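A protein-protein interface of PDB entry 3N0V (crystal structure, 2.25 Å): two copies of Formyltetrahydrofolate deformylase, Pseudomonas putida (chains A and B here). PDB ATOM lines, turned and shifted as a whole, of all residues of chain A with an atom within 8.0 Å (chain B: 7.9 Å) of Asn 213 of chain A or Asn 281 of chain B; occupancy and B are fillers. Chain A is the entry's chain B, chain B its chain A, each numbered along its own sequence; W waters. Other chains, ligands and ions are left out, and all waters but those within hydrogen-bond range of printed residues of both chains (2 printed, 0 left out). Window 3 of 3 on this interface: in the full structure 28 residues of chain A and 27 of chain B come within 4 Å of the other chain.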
ATOM      1  N   PHE A 202     -16.203  15.777 -14.072  1.00  0.00           N
ATOM      2  CA  PHE A 202     -17.466  16.524 -14.112  1.00  0.00           C
ATOM      3  C   PHE A 202     -18.273  16.360 -12.828  1.00  0.00           C
ATOM      4  O   PHE A 202     -18.175  15.336 -12.158  1.00  0.00           O
ATOM      5  CB  PHE A 202     -18.319  16.074 -15.298  1.00  0.00           C
ATOM      6  CG  PHE A 202     -17.541  15.910 -16.559  1.00  0.00           C
ATOM      7  CD1 PHE A 202     -16.996  17.015 -17.190  1.00  0.00           C
ATOM      8  CD2 PHE A 202     -17.332  14.653 -17.103  1.00  0.00           C
ATOM      9  CE1 PHE A 202     -16.261  16.870 -18.348  1.00  0.00           C
ATOM     10  CE2 PHE A 202     -16.601  14.501 -18.262  1.00  0.00           C
ATOM     11  CZ  PHE A 202     -16.059  15.607 -18.886  1.00  0.00           C
ATOM     12  N   LYS A 206     -25.911  17.655 -16.006  1.00  0.00           N
ATOM     13  CA  LYS A 206     -25.866  16.668 -17.076  1.00  0.00           C
ATOM     14  C   LYS A 206     -24.428  16.199 -17.331  1.00  0.00           C
ATOM     15  O   LYS A 206     -23.686  16.855 -18.070  1.00  0.00           O
ATOM     16  CB  LYS A 206     -26.490  17.251 -18.346  1.00  0.00           C
ATOM     17  CG  LYS A 206     -28.008  17.384 -18.252  1.00  0.00           C
ATOM     18  CD  LYS A 206     -28.642  17.809 -19.571  1.00  0.00           C
ATOM     19  CE  LYS A 206     -30.163  17.735 -19.505  1.00  0.00           C
ATOM     20  NZ  LYS A 206     -30.651  16.376 -19.128  1.00  0.00           N
ATOM     21  N   PRO A 207     -24.026  15.064 -16.717  1.00  0.00           N
ATOM     22  CA  PRO A 207     -22.606  14.676 -16.756  1.00  0.00           C
ATOM     23  C   PRO A 207     -22.140  14.206 -18.138  1.00  0.00           C
ATOM     24  O   PRO A 207     -21.020  14.517 -18.557  1.00  0.00           O
ATOM     25  CB  PRO A 207     -22.517  13.520 -15.744  1.00  0.00           C
ATOM     26  CG  PRO A 207     -23.839  13.491 -15.047  1.00  0.00           C
ATOM     27  CD  PRO A 207     -24.826  14.067 -15.987  1.00  0.00           C
ATOM     28  N   TYR A 208     -23.003  13.476 -18.834  1.00  0.00           N
ATOM     29  CA  TYR A 208     -22.700  13.003 -20.181  1.00  0.00           C
ATOM     30  C   TYR A 208     -22.659  14.146 -21.197  1.00  0.00           C
ATOM     31  O   TYR A 208     -21.862  14.126 -22.134  1.00  0.00           O
ATOM     32  CB  TYR A 208     -23.693  11.908 -20.597  1.00  0.00           C
ATOM     33  CG  TYR A 208     -23.467  10.619 -19.842  1.00  0.00           C
ATOM     34  CD1 TYR A 208     -22.408   9.802 -20.163  1.00  0.00           C
ATOM     35  CD2 TYR A 208     -24.292  10.238 -18.783  1.00  0.00           C
ATOM     36  CE1 TYR A 208     -22.171   8.621 -19.483  1.00  0.00           C
ATOM     37  CE2 TYR A 208     -24.065   9.044 -18.085  1.00  0.00           C
ATOM     38  CZ  TYR A 208     -22.997   8.239 -18.453  1.00  0.00           C
ATOM     39  OH  TYR A 208     -22.722   7.057 -17.802  1.00  0.00           O
ATOM     40  N   HIS A 209     -23.494  15.158 -20.999  1.00  0.00           N
ATOM     41  CA  HIS A 209     -23.471  16.332 -21.869  1.00  0.00           C
ATOM     42  C   HIS A 209     -22.157  17.093 -21.666  1.00  0.00           C
ATOM     43  O   HIS A 209     -21.569  17.576 -22.633  1.00  0.00           O
ATOM     44  CB  HIS A 209     -24.680  17.237 -21.625  1.00  0.00           C
ATOM     45  CG  HIS A 209     -25.989  16.616 -22.015  1.00  0.00           C
ATOM     46  ND1 HIS A 209     -26.515  15.512 -21.374  1.00  0.00           N
ATOM     47  CD2 HIS A 209     -26.882  16.950 -22.980  1.00  0.00           C
ATOM     48  CE1 HIS A 209     -27.670  15.190 -21.931  1.00  0.00           C
ATOM     49  NE2 HIS A 209     -27.915  16.043 -22.910  1.00  0.00           N
ATOM     50  N   GLN A 210     -21.697  17.173 -20.415  1.00  0.00           N
ATOM     51  CA  GLN A 210     -20.394  17.772 -20.100  1.00  0.00           C
ATOM     52  C   GLN A 210     -19.238  16.946 -20.665  1.00  0.00           C
ATOM     53  O   GLN A 210     -18.228  17.511 -21.066  1.00  0.00           O
ATOM     54  CB  GLN A 210     -20.200  17.930 -18.590  1.00  0.00           C
ATOM     55  CG  GLN A 210     -21.014  19.029 -17.964  1.00  0.00           C
ATOM     56  CD  GLN A 210     -20.753  19.152 -16.485  1.00  0.00           C
ATOM     57  OE1 GLN A 210     -21.517  18.651 -15.663  1.00  0.00           O
ATOM     58  NE2 GLN A 210     -19.655  19.806 -16.134  1.00  0.00           N
ATOM     59  N   ALA A 211     -19.382  15.618 -20.678  1.00  0.00           N
ATOM     60  CA  ALA A 211     -18.390  14.740 -21.320  1.00  0.00           C
ATOM     61  C   ALA A 211     -18.334  15.006 -22.821  1.00  0.00           C
ATOM     62  O   ALA A 211     -17.247  15.187 -23.374  1.00  0.00           O
ATOM     63  CB  ALA A 211     -18.688  13.264 -21.052  1.00  0.00           C
ATOM     64  N   TYR A 212     -19.497  15.043 -23.471  1.00  0.00           N
ATOM     65  CA  TYR A 212     -19.558  15.330 -24.908  1.00  0.00           C
ATOM     66  C   TYR A 212     -18.807  16.615 -25.249  1.00  0.00           C
ATOM     67  O   TYR A 212     -17.934  16.607 -26.114  1.00  0.00           O
ATOM     68  CB  TYR A 212     -21.004  15.415 -25.419  1.00  0.00           C
ATOM     69  CG  TYR A 212     -21.081  15.777 -26.882  1.00  0.00           C
ATOM     70  CD1 TYR A 212     -20.698  14.862 -27.848  1.00  0.00           C
ATOM     71  CD2 TYR A 212     -21.522  17.043 -27.305  1.00  0.00           C
ATOM     72  CE1 TYR A 212     -20.744  15.177 -29.216  1.00  0.00           C
ATOM     73  CE2 TYR A 212     -21.577  17.370 -28.682  1.00  0.00           C
ATOM     74  CZ  TYR A 212     -21.171  16.422 -29.631  1.00  0.00           C
ATOM     75  OH  TYR A 212     -21.200  16.677 -30.994  1.00  0.00           O
ATOM     76  N   ASN A 213     -19.140  17.705 -24.558  1.00  0.00           N
ATOM     77  CA  ASN A 213     -18.512  19.010 -24.809  1.00  0.00           C
ATOM     78  C   ASN A 213     -17.000  19.022 -24.557  1.00  0.00           C
ATOM     79  O   ASN A 213     -16.270  19.725 -25.246  1.00  0.00           O
ATOM     80  CB  ASN A 213     -19.175  20.122 -23.966  1.00  0.00           C
ATOM     81  CG  ASN A 213     -20.596  20.473 -24.435  1.00  0.00           C
ATOM     82  OD1 ASN A 213     -20.909  20.446 -25.625  1.00  0.00           O
ATOM     83  ND2 ASN A 213     -21.447  20.824 -23.488  1.00  0.00           N
ATOM     84  N   LYS A 214     -16.547  18.261 -23.562  1.00  0.00           N
ATOM     85  CA  LYS A 214     -15.124  18.197 -23.184  1.00  0.00           C
ATOM     86  C   LYS A 214     -14.339  17.355 -24.209  1.00  0.00           C
ATOM     87  O   LYS A 214     -13.123  17.519 -24.378  1.00  0.00           O
ATOM     88  CB  LYS A 214     -14.992  17.627 -21.761  1.00  0.00           C
ATOM     89  CG  LYS A 214     -13.579  17.518 -21.184  1.00  0.00           C
ATOM     90  CD  LYS A 214     -12.859  18.871 -21.195  1.00  0.00           C
ATOM     91  CE  LYS A 214     -11.533  18.815 -20.478  1.00  0.00           C
ATOM     92  NZ  LYS A 214     -10.645  19.888 -20.978  1.00  0.00           N
ATOM     93  N   GLY A 215     -15.063  16.468 -24.890  1.00  0.00           N
ATOM     94  CA  GLY A 215     -14.544  15.691 -25.995  1.00  0.00           C
ATOM     95  C   GLY A 215     -13.905  14.397 -25.557  1.00  0.00           C
ATOM     96  O   GLY A 215     -12.976  13.935 -26.187  1.00  0.00           O
ATOM     97  N   VAL A 216     -14.394  13.809 -24.475  1.00  0.00           N
ATOM     98  CA  VAL A 216     -13.789  12.588 -23.926  1.00  0.00           C
ATOM     99  C   VAL A 216     -13.841  11.456 -24.945  1.00  0.00           C
ATOM    100  O   VAL A 216     -14.673  11.457 -25.844  1.00  0.00           O
ATOM    101  CB  VAL A 216     -14.461  12.128 -22.593  1.00  0.00           C
ATOM    102  CG1 VAL A 216     -14.308  13.179 -21.519  1.00  0.00           C
ATOM    103  CG2 VAL A 216     -15.944  11.774 -22.788  1.00  0.00           C
ATOM    104  N   HIS A 247     -20.347   9.910 -31.176  1.00  0.00           N
ATOM    105  CA  HIS A 247     -21.233   9.687 -30.045  1.00  0.00           C
ATOM    106  C   HIS A 247     -21.767  11.007 -29.488  1.00  0.00           C
ATOM    107  O   HIS A 247     -21.075  11.729 -28.761  1.00  0.00           O
ATOM    108  CB  HIS A 247     -20.508   8.908 -28.951  1.00  0.00           C
ATOM    109  CG  HIS A 247     -20.222   7.490 -29.320  1.00  0.00           C
ATOM    110  ND1 HIS A 247     -19.111   7.120 -30.044  1.00  0.00           N
ATOM    111  CD2 HIS A 247     -20.904   6.348 -29.066  1.00  0.00           C
ATOM    112  CE1 HIS A 247     -19.118   5.811 -30.222  1.00  0.00           C
ATOM    113  NE2 HIS A 247     -20.195   5.319 -29.638  1.00  0.00           N
ATOM    114  N   PRO A 249     -24.522  13.189 -27.035  1.00  0.00           N
ATOM    115  CA  PRO A 249     -24.815  12.934 -25.618  1.00  0.00           C
ATOM    116  C   PRO A 249     -25.660  11.681 -25.333  1.00  0.00           C
ATOM    117  O   PRO A 249     -25.317  10.921 -24.420  1.00  0.00           O
ATOM    118  CB  PRO A 249     -25.542  14.211 -25.187  1.00  0.00           C
ATOM    119  CG  PRO A 249     -24.906  15.264 -26.006  1.00  0.00           C
ATOM    120  CD  PRO A 249     -24.668  14.622 -27.357  1.00  0.00           C
ATOM    121  N   LEU A 252     -23.745   8.705 -25.691  1.00  0.00           N
ATOM    122  CA  LEU A 252     -22.822   8.659 -24.563  1.00  0.00           C
ATOM    123  C   LEU A 252     -23.499   7.993 -23.366  1.00  0.00           C
ATOM    124  O   LEU A 252     -22.929   7.125 -22.709  1.00  0.00           O
ATOM    125  CB  LEU A 252     -22.368  10.082 -24.207  1.00  0.00           C
ATOM    126  CG  LEU A 252     -20.865  10.334 -24.182  1.00  0.00           C
ATOM    127  CD1 LEU A 252     -20.550  11.747 -24.664  1.00  0.00           C
ATOM    128  CD2 LEU A 252     -20.307  10.100 -22.796  1.00  0.00           C
ATOM    129  N   GLN B  46     -23.985  19.394 -33.424  1.00  0.00           N
ATOM    130  CA  GLN B  46     -23.945  20.317 -32.283  1.00  0.00           C
ATOM    131  C   GLN B  46     -23.025  21.507 -32.576  1.00  0.00           C
ATOM    132  O   GLN B  46     -23.399  22.643 -32.288  1.00  0.00           O
ATOM    133  CB  GLN B  46     -23.506  19.615 -30.998  1.00  0.00           C
ATOM    134  CG  GLN B  46     -24.283  18.330 -30.690  1.00  0.00           C
ATOM    135  CD  GLN B  46     -25.348  18.462 -29.602  1.00  0.00           C
ATOM    136  OE1 GLN B  46     -26.444  17.916 -29.743  1.00  0.00           O
ATOM    137  NE2 GLN B  46     -25.017  19.149 -28.500  1.00  0.00           N
ATOM    138  N   SER B  47     -21.843  21.251 -33.149  1.00  0.00           N
ATOM    139  CA  SER B  47     -20.865  22.316 -33.437  1.00  0.00           C
ATOM    140  C   SER B  47     -21.060  23.030 -34.783  1.00  0.00           C
ATOM    141  O   SER B  47     -20.446  24.057 -35.016  1.00  0.00           O
ATOM    142  CB  SER B  47     -19.431  21.792 -33.362  1.00  0.00           C
ATOM    143  OG  SER B  47     -19.135  20.904 -34.442  1.00  0.00           O
ATOM    144  N   ASN B 227      -2.806  24.235 -25.517  1.00  0.00           N
ATOM    145  CA  ASN B 227      -3.357  25.590 -25.557  1.00  0.00           C
ATOM    146  C   ASN B 227      -3.078  26.274 -24.199  1.00  0.00           C
ATOM    147  O   ASN B 227      -2.277  25.762 -23.413  1.00  0.00           O
ATOM    148  CB  ASN B 227      -4.855  25.575 -25.941  1.00  0.00           C
ATOM    149  CG  ASN B 227      -5.779  25.123 -24.798  1.00  0.00           C
ATOM    150  OD1 ASN B 227      -5.366  24.992 -23.650  1.00  0.00           O
ATOM    151  ND2 ASN B 227      -7.043  24.895 -25.126  1.00  0.00           N
ATOM    152  N   ASP B 229      -4.894  26.593 -21.499  1.00  0.00           N
ATOM    153  CA  ASP B 229      -5.379  25.834 -20.343  1.00  0.00           C
ATOM    154  C   ASP B 229      -4.405  24.699 -20.037  1.00  0.00           C
ATOM    155  O   ASP B 229      -4.307  23.751 -20.813  1.00  0.00           O
ATOM    156  CB  ASP B 229      -6.778  25.254 -20.608  1.00  0.00           C
ATOM    157  CG  ASP B 229      -7.829  26.328 -20.842  1.00  0.00           C
ATOM    158  OD1 ASP B 229      -7.952  27.241 -19.995  1.00  0.00           O
ATOM    159  OD2 ASP B 229      -8.541  26.254 -21.868  1.00  0.00           O
ATOM    160  N   GLU B 232      -5.298  20.752 -19.868  1.00  0.00           N
ATOM    161  CA  GLU B 232      -6.569  20.625 -20.540  1.00  0.00           C
ATOM    162  C   GLU B 232      -6.269  21.103 -21.945  1.00  0.00           C
ATOM    163  O   GLU B 232      -5.111  21.262 -22.308  1.00  0.00           O
ATOM    164  CB  GLU B 232      -7.640  21.494 -19.867  1.00  0.00           C
ATOM    165  CG  GLU B 232      -7.637  21.496 -18.322  1.00  0.00           C
ATOM    166  CD  GLU B 232      -7.686  20.104 -17.679  1.00  0.00           C
ATOM    167  OE1 GLU B 232      -8.171  19.142 -18.303  1.00  0.00           O
ATOM    168  OE2 GLU B 232      -7.247  19.980 -16.517  1.00  0.00           O
ATOM    169  N   GLY B 233      -7.284  21.369 -22.744  1.00  0.00           N
ATOM    170  CA  GLY B 233      -7.025  21.643 -24.153  1.00  0.00           C
ATOM    171  C   GLY B 233      -7.325  20.392 -24.941  1.00  0.00           C
ATOM    172  O   GLY B 233      -7.447  19.315 -24.358  1.00  0.00           O
ATOM    173  N   PRO B 234      -7.433  20.523 -26.271  1.00  0.00           N
ATOM    174  CA  PRO B 234      -8.136  19.538 -27.095  1.00  0.00           C
ATOM    175  C   PRO B 234      -7.660  18.083 -26.943  1.00  0.00           C
ATOM    176  O   PRO B 234      -6.525  17.748 -27.294  1.00  0.00           O
ATOM    177  CB  PRO B 234      -7.908  20.056 -28.517  1.00  0.00           C
ATOM    178  CG  PRO B 234      -7.693  21.505 -28.358  1.00  0.00           C
ATOM    179  CD  PRO B 234      -6.933  21.648 -27.078  1.00  0.00           C
ATOM    180  N   ILE B 235      -8.541  17.231 -26.428  1.00  0.00           N
ATOM    181  CA  ILE B 235      -8.241  15.815 -26.241  1.00  0.00           C
ATOM    182  C   ILE B 235      -8.188  15.070 -27.583  1.00  0.00           C
ATOM    183  O   ILE B 235      -9.142  15.119 -28.359  1.00  0.00           O
ATOM    184  CB  ILE B 235      -9.284  15.148 -25.323  1.00  0.00           C
ATOM    185  CG1 ILE B 235      -9.261  15.763 -23.921  1.00  0.00           C
ATOM    186  CG2 ILE B 235      -9.027  13.663 -25.202  1.00  0.00           C
ATOM    187  CD1 ILE B 235     -10.436  15.354 -23.080  1.00  0.00           C
ATOM    188  N   PHE B 277      -8.776  16.577 -36.549  1.00  0.00           N
ATOM    189  CA  PHE B 277      -9.283  17.932 -36.813  1.00  0.00           C
ATOM    190  C   PHE B 277      -9.669  18.558 -35.486  1.00  0.00           C
ATOM    191  O   PHE B 277     -10.140  17.857 -34.584  1.00  0.00           O
ATOM    192  CB  PHE B 277     -10.546  17.889 -37.667  1.00  0.00           C
ATOM    193  CG  PHE B 277     -10.391  17.174 -38.967  1.00  0.00           C
ATOM    194  CD1 PHE B 277     -10.237  15.795 -39.003  1.00  0.00           C
ATOM    195  CD2 PHE B 277     -10.423  17.874 -40.166  1.00  0.00           C
ATOM    196  CE1 PHE B 277     -10.107  15.130 -40.201  1.00  0.00           C
ATOM    197  CE2 PHE B 277     -10.296  17.211 -41.369  1.00  0.00           C
ATOM    198  CZ  PHE B 277     -10.140  15.838 -41.389  1.00  0.00           C
ATOM    199  N   LEU B 278      -9.487  19.871 -35.377  1.00  0.00           N
ATOM    200  CA  LEU B 278      -9.983  20.640 -34.244  1.00  0.00           C
ATOM    201  C   LEU B 278     -11.449  20.963 -34.499  1.00  0.00           C
ATOM    202  O   LEU B 278     -11.813  21.391 -35.583  1.00  0.00           O
ATOM    203  CB  LEU B 278      -9.192  21.943 -34.079  1.00  0.00           C
ATOM    204  CG  LEU B 278      -7.705  21.832 -33.733  1.00  0.00           C
ATOM    205  CD1 LEU B 278      -7.024  23.193 -33.869  1.00  0.00           C
ATOM    206  CD2 LEU B 278      -7.518  21.262 -32.323  1.00  0.00           C
ATOM    207  N   ASN B 279     -12.283  20.753 -33.500  1.00  0.00           N
ATOM    208  CA  ASN B 279     -13.726  20.935 -33.626  1.00  0.00           C
ATOM    209  C   ASN B 279     -14.206  21.650 -32.381  1.00  0.00           C
ATOM    210  O   ASN B 279     -14.401  21.020 -31.356  1.00  0.00           O
ATOM    211  CB  ASN B 279     -14.391  19.558 -33.761  1.00  0.00           C
ATOM    212  CG  ASN B 279     -15.910  19.620 -33.777  1.00  0.00           C
ATOM    213  OD1 ASN B 279     -16.515  20.625 -34.168  1.00  0.00           O
ATOM    214  ND2 ASN B 279     -16.537  18.522 -33.353  1.00  0.00           N
ATOM    215  N   ALA B 280     -14.383  22.969 -32.480  1.00  0.00           N
ATOM    216  CA  ALA B 280     -14.527  23.851 -31.319  1.00  0.00           C
ATOM    217  C   ALA B 280     -13.354  23.596 -30.342  1.00  0.00           C
ATOM    218  O   ALA B 280     -12.212  23.886 -30.681  1.00  0.00           O
ATOM    219  CB  ALA B 280     -15.888  23.679 -30.664  1.00  0.00           C
ATOM    220  N   ASN B 281     -13.620  23.033 -29.168  1.00  0.00           N
ATOM    221  CA  ASN B 281     -12.589  22.800 -28.154  1.00  0.00           C
ATOM    222  C   ASN B 281     -12.222  21.304 -28.031  1.00  0.00           C
ATOM    223  O   ASN B 281     -11.609  20.887 -27.048  1.00  0.00           O
ATOM    224  CB  ASN B 281     -13.101  23.293 -26.797  1.00  0.00           C
ATOM    225  CG  ASN B 281     -14.321  22.502 -26.314  1.00  0.00           C
ATOM    226  OD1 ASN B 281     -15.260  22.267 -27.079  1.00  0.00           O
ATOM    227  ND2 ASN B 281     -14.298  22.073 -25.057  1.00  0.00           N
ATOM    228  N   ARG B 282     -12.621  20.502 -29.017  1.00  0.00           N
ATOM    229  CA  ARG B 282     -12.390  19.057 -29.004  1.00  0.00           C
ATOM    230  C   ARG B 282     -11.830  18.573 -30.353  1.00  0.00           C
ATOM    231  O   ARG B 282     -11.454  19.379 -31.193  1.00  0.00           O
ATOM    232  CB  ARG B 282     -13.681  18.315 -28.618  1.00  0.00           C
ATOM    233  CG  ARG B 282     -14.965  18.868 -29.204  1.00  0.00           C
ATOM    234  CD  ARG B 282     -16.182  18.155 -28.634  1.00  0.00           C
ATOM    235  NE  ARG B 282     -17.341  18.226 -29.529  1.00  0.00           N
ATOM    236  CZ  ARG B 282     -18.232  19.217 -29.566  1.00  0.00           C
ATOM    237  NH1 ARG B 282     -18.118  20.276 -28.765  1.00  0.00           N
ATOM    238  NH2 ARG B 282     -19.248  19.151 -30.422  1.00  0.00           N
ATOM    239  N   THR B 283     -11.723  17.261 -30.546  1.00  0.00           N
ATOM    240  CA  THR B 283     -11.198  16.736 -31.797  1.00  0.00           C
ATOM    241  C   THR B 283     -12.129  15.713 -32.401  1.00  0.00           C
ATOM    242  O   THR B 283     -12.804  14.973 -31.683  1.00  0.00           O
ATOM    243  CB  THR B 283      -9.838  16.043 -31.631  1.00  0.00           C
ATOM    244  OG1 THR B 283      -9.983  14.898 -30.780  1.00  0.00           O
ATOM    245  CG2 THR B 283      -8.814  16.992 -31.070  1.00  0.00           C
HETATM  246  O   HOH W   1     -11.864  15.508 -28.025  1.00  0.00           O
HETATM  247  O   HOH W   2     -11.080  18.572 -25.606  1.00  0.00           O
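No position is printed for both chains. Of the 8 pairs that touch across the chains among the printed residues, none has its exchanged pair printed and touching as well.
Water W2 lies within hydrogen-bond range of O of Lys 214 of chain A, O of Asn 281 of chain B and N of Ile 235 of chain B. Water W1 lies within hydrogen-bond range of the backbone carbonyl oxygen (O) of Gly 215 of chain A, the backbone carbonyl oxygen (O) of Ile 235 of chain B and the backbone NH (N) of Thr 283 of chain B.
Of the 15 printed residues of chain B, 5 touch a printed residue of chain A. Hydrophobic or aromatic side chains of chain A within 4 Å of the printed part of chain B: Tyr 212. Among the printed residues, Asp or Glu carboxylates within 4 Å of a Lys or Arg side-chain nitrogen of the other chain: Lys 214 of chain A with Glu 232 of chain B (3.7 Å).
Asn 213 of chain A touches just these residues of chain B: Asn 281 (3.1 Å) and Arg 282 (3.7 Å). Of the printed residues of chain B, Lys 214 of chain A touches Glu 232 and Ile 235. Of the printed residues of chain A, Glu 232 of chain B touches Lys 214. Leu 278 of chain B touches none of the printed residues of chain A. No residue of chain A comes within 4 Å of Ala 280 of chain B. Asn 281 of chain B touches one residue of chain A. The nearest residue of chain A that does not touch Asn 281 of chain B is Lys 214 of chain A (4.4 Å). The nearest printed residue of chain A that does not touch Gln 46 of chain B is Pro 249 of chain A (4.4 Å).
O of Ile 235 of chain B lies within hydrogen-bond range of OG1 of Thr 283 of chain B. O of His 209 of chain A is in hydrogen-bond range of ND2 of Asn 213 of chain A.
The side-chain carboxylate (OE1) of Glu 232 of chain B is in salt-bridge range of the side-chain amino group (NZ) of Lys 214 of chain A (3.7 Å). O of Asn 213 of chain A lies within hydrogen-bond range of ND2 of Asn 281 of chain B. OH of Tyr 212 of chain A sits at hydrogen-bond distance from NH2 of Arg 282 of chain B (3.2 Å).
CE2 of Tyr 212 of chain A touches CG of Gln 46 of chain B, at 3.5 Å. Arg 282 of chain B touches Asn 213 of chain A (CD to O, 3.7 Å). CD1 of Ile 235 of chain B touches O of Lys 214 of chain A, at 3.7 Å. O of Gly 215 of chain A touches CB of Ile 235 of chain B (3.98 Å). Arg 282 of chain B touches Gly 215 of chain A (CB to CA, 3.8 Å).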
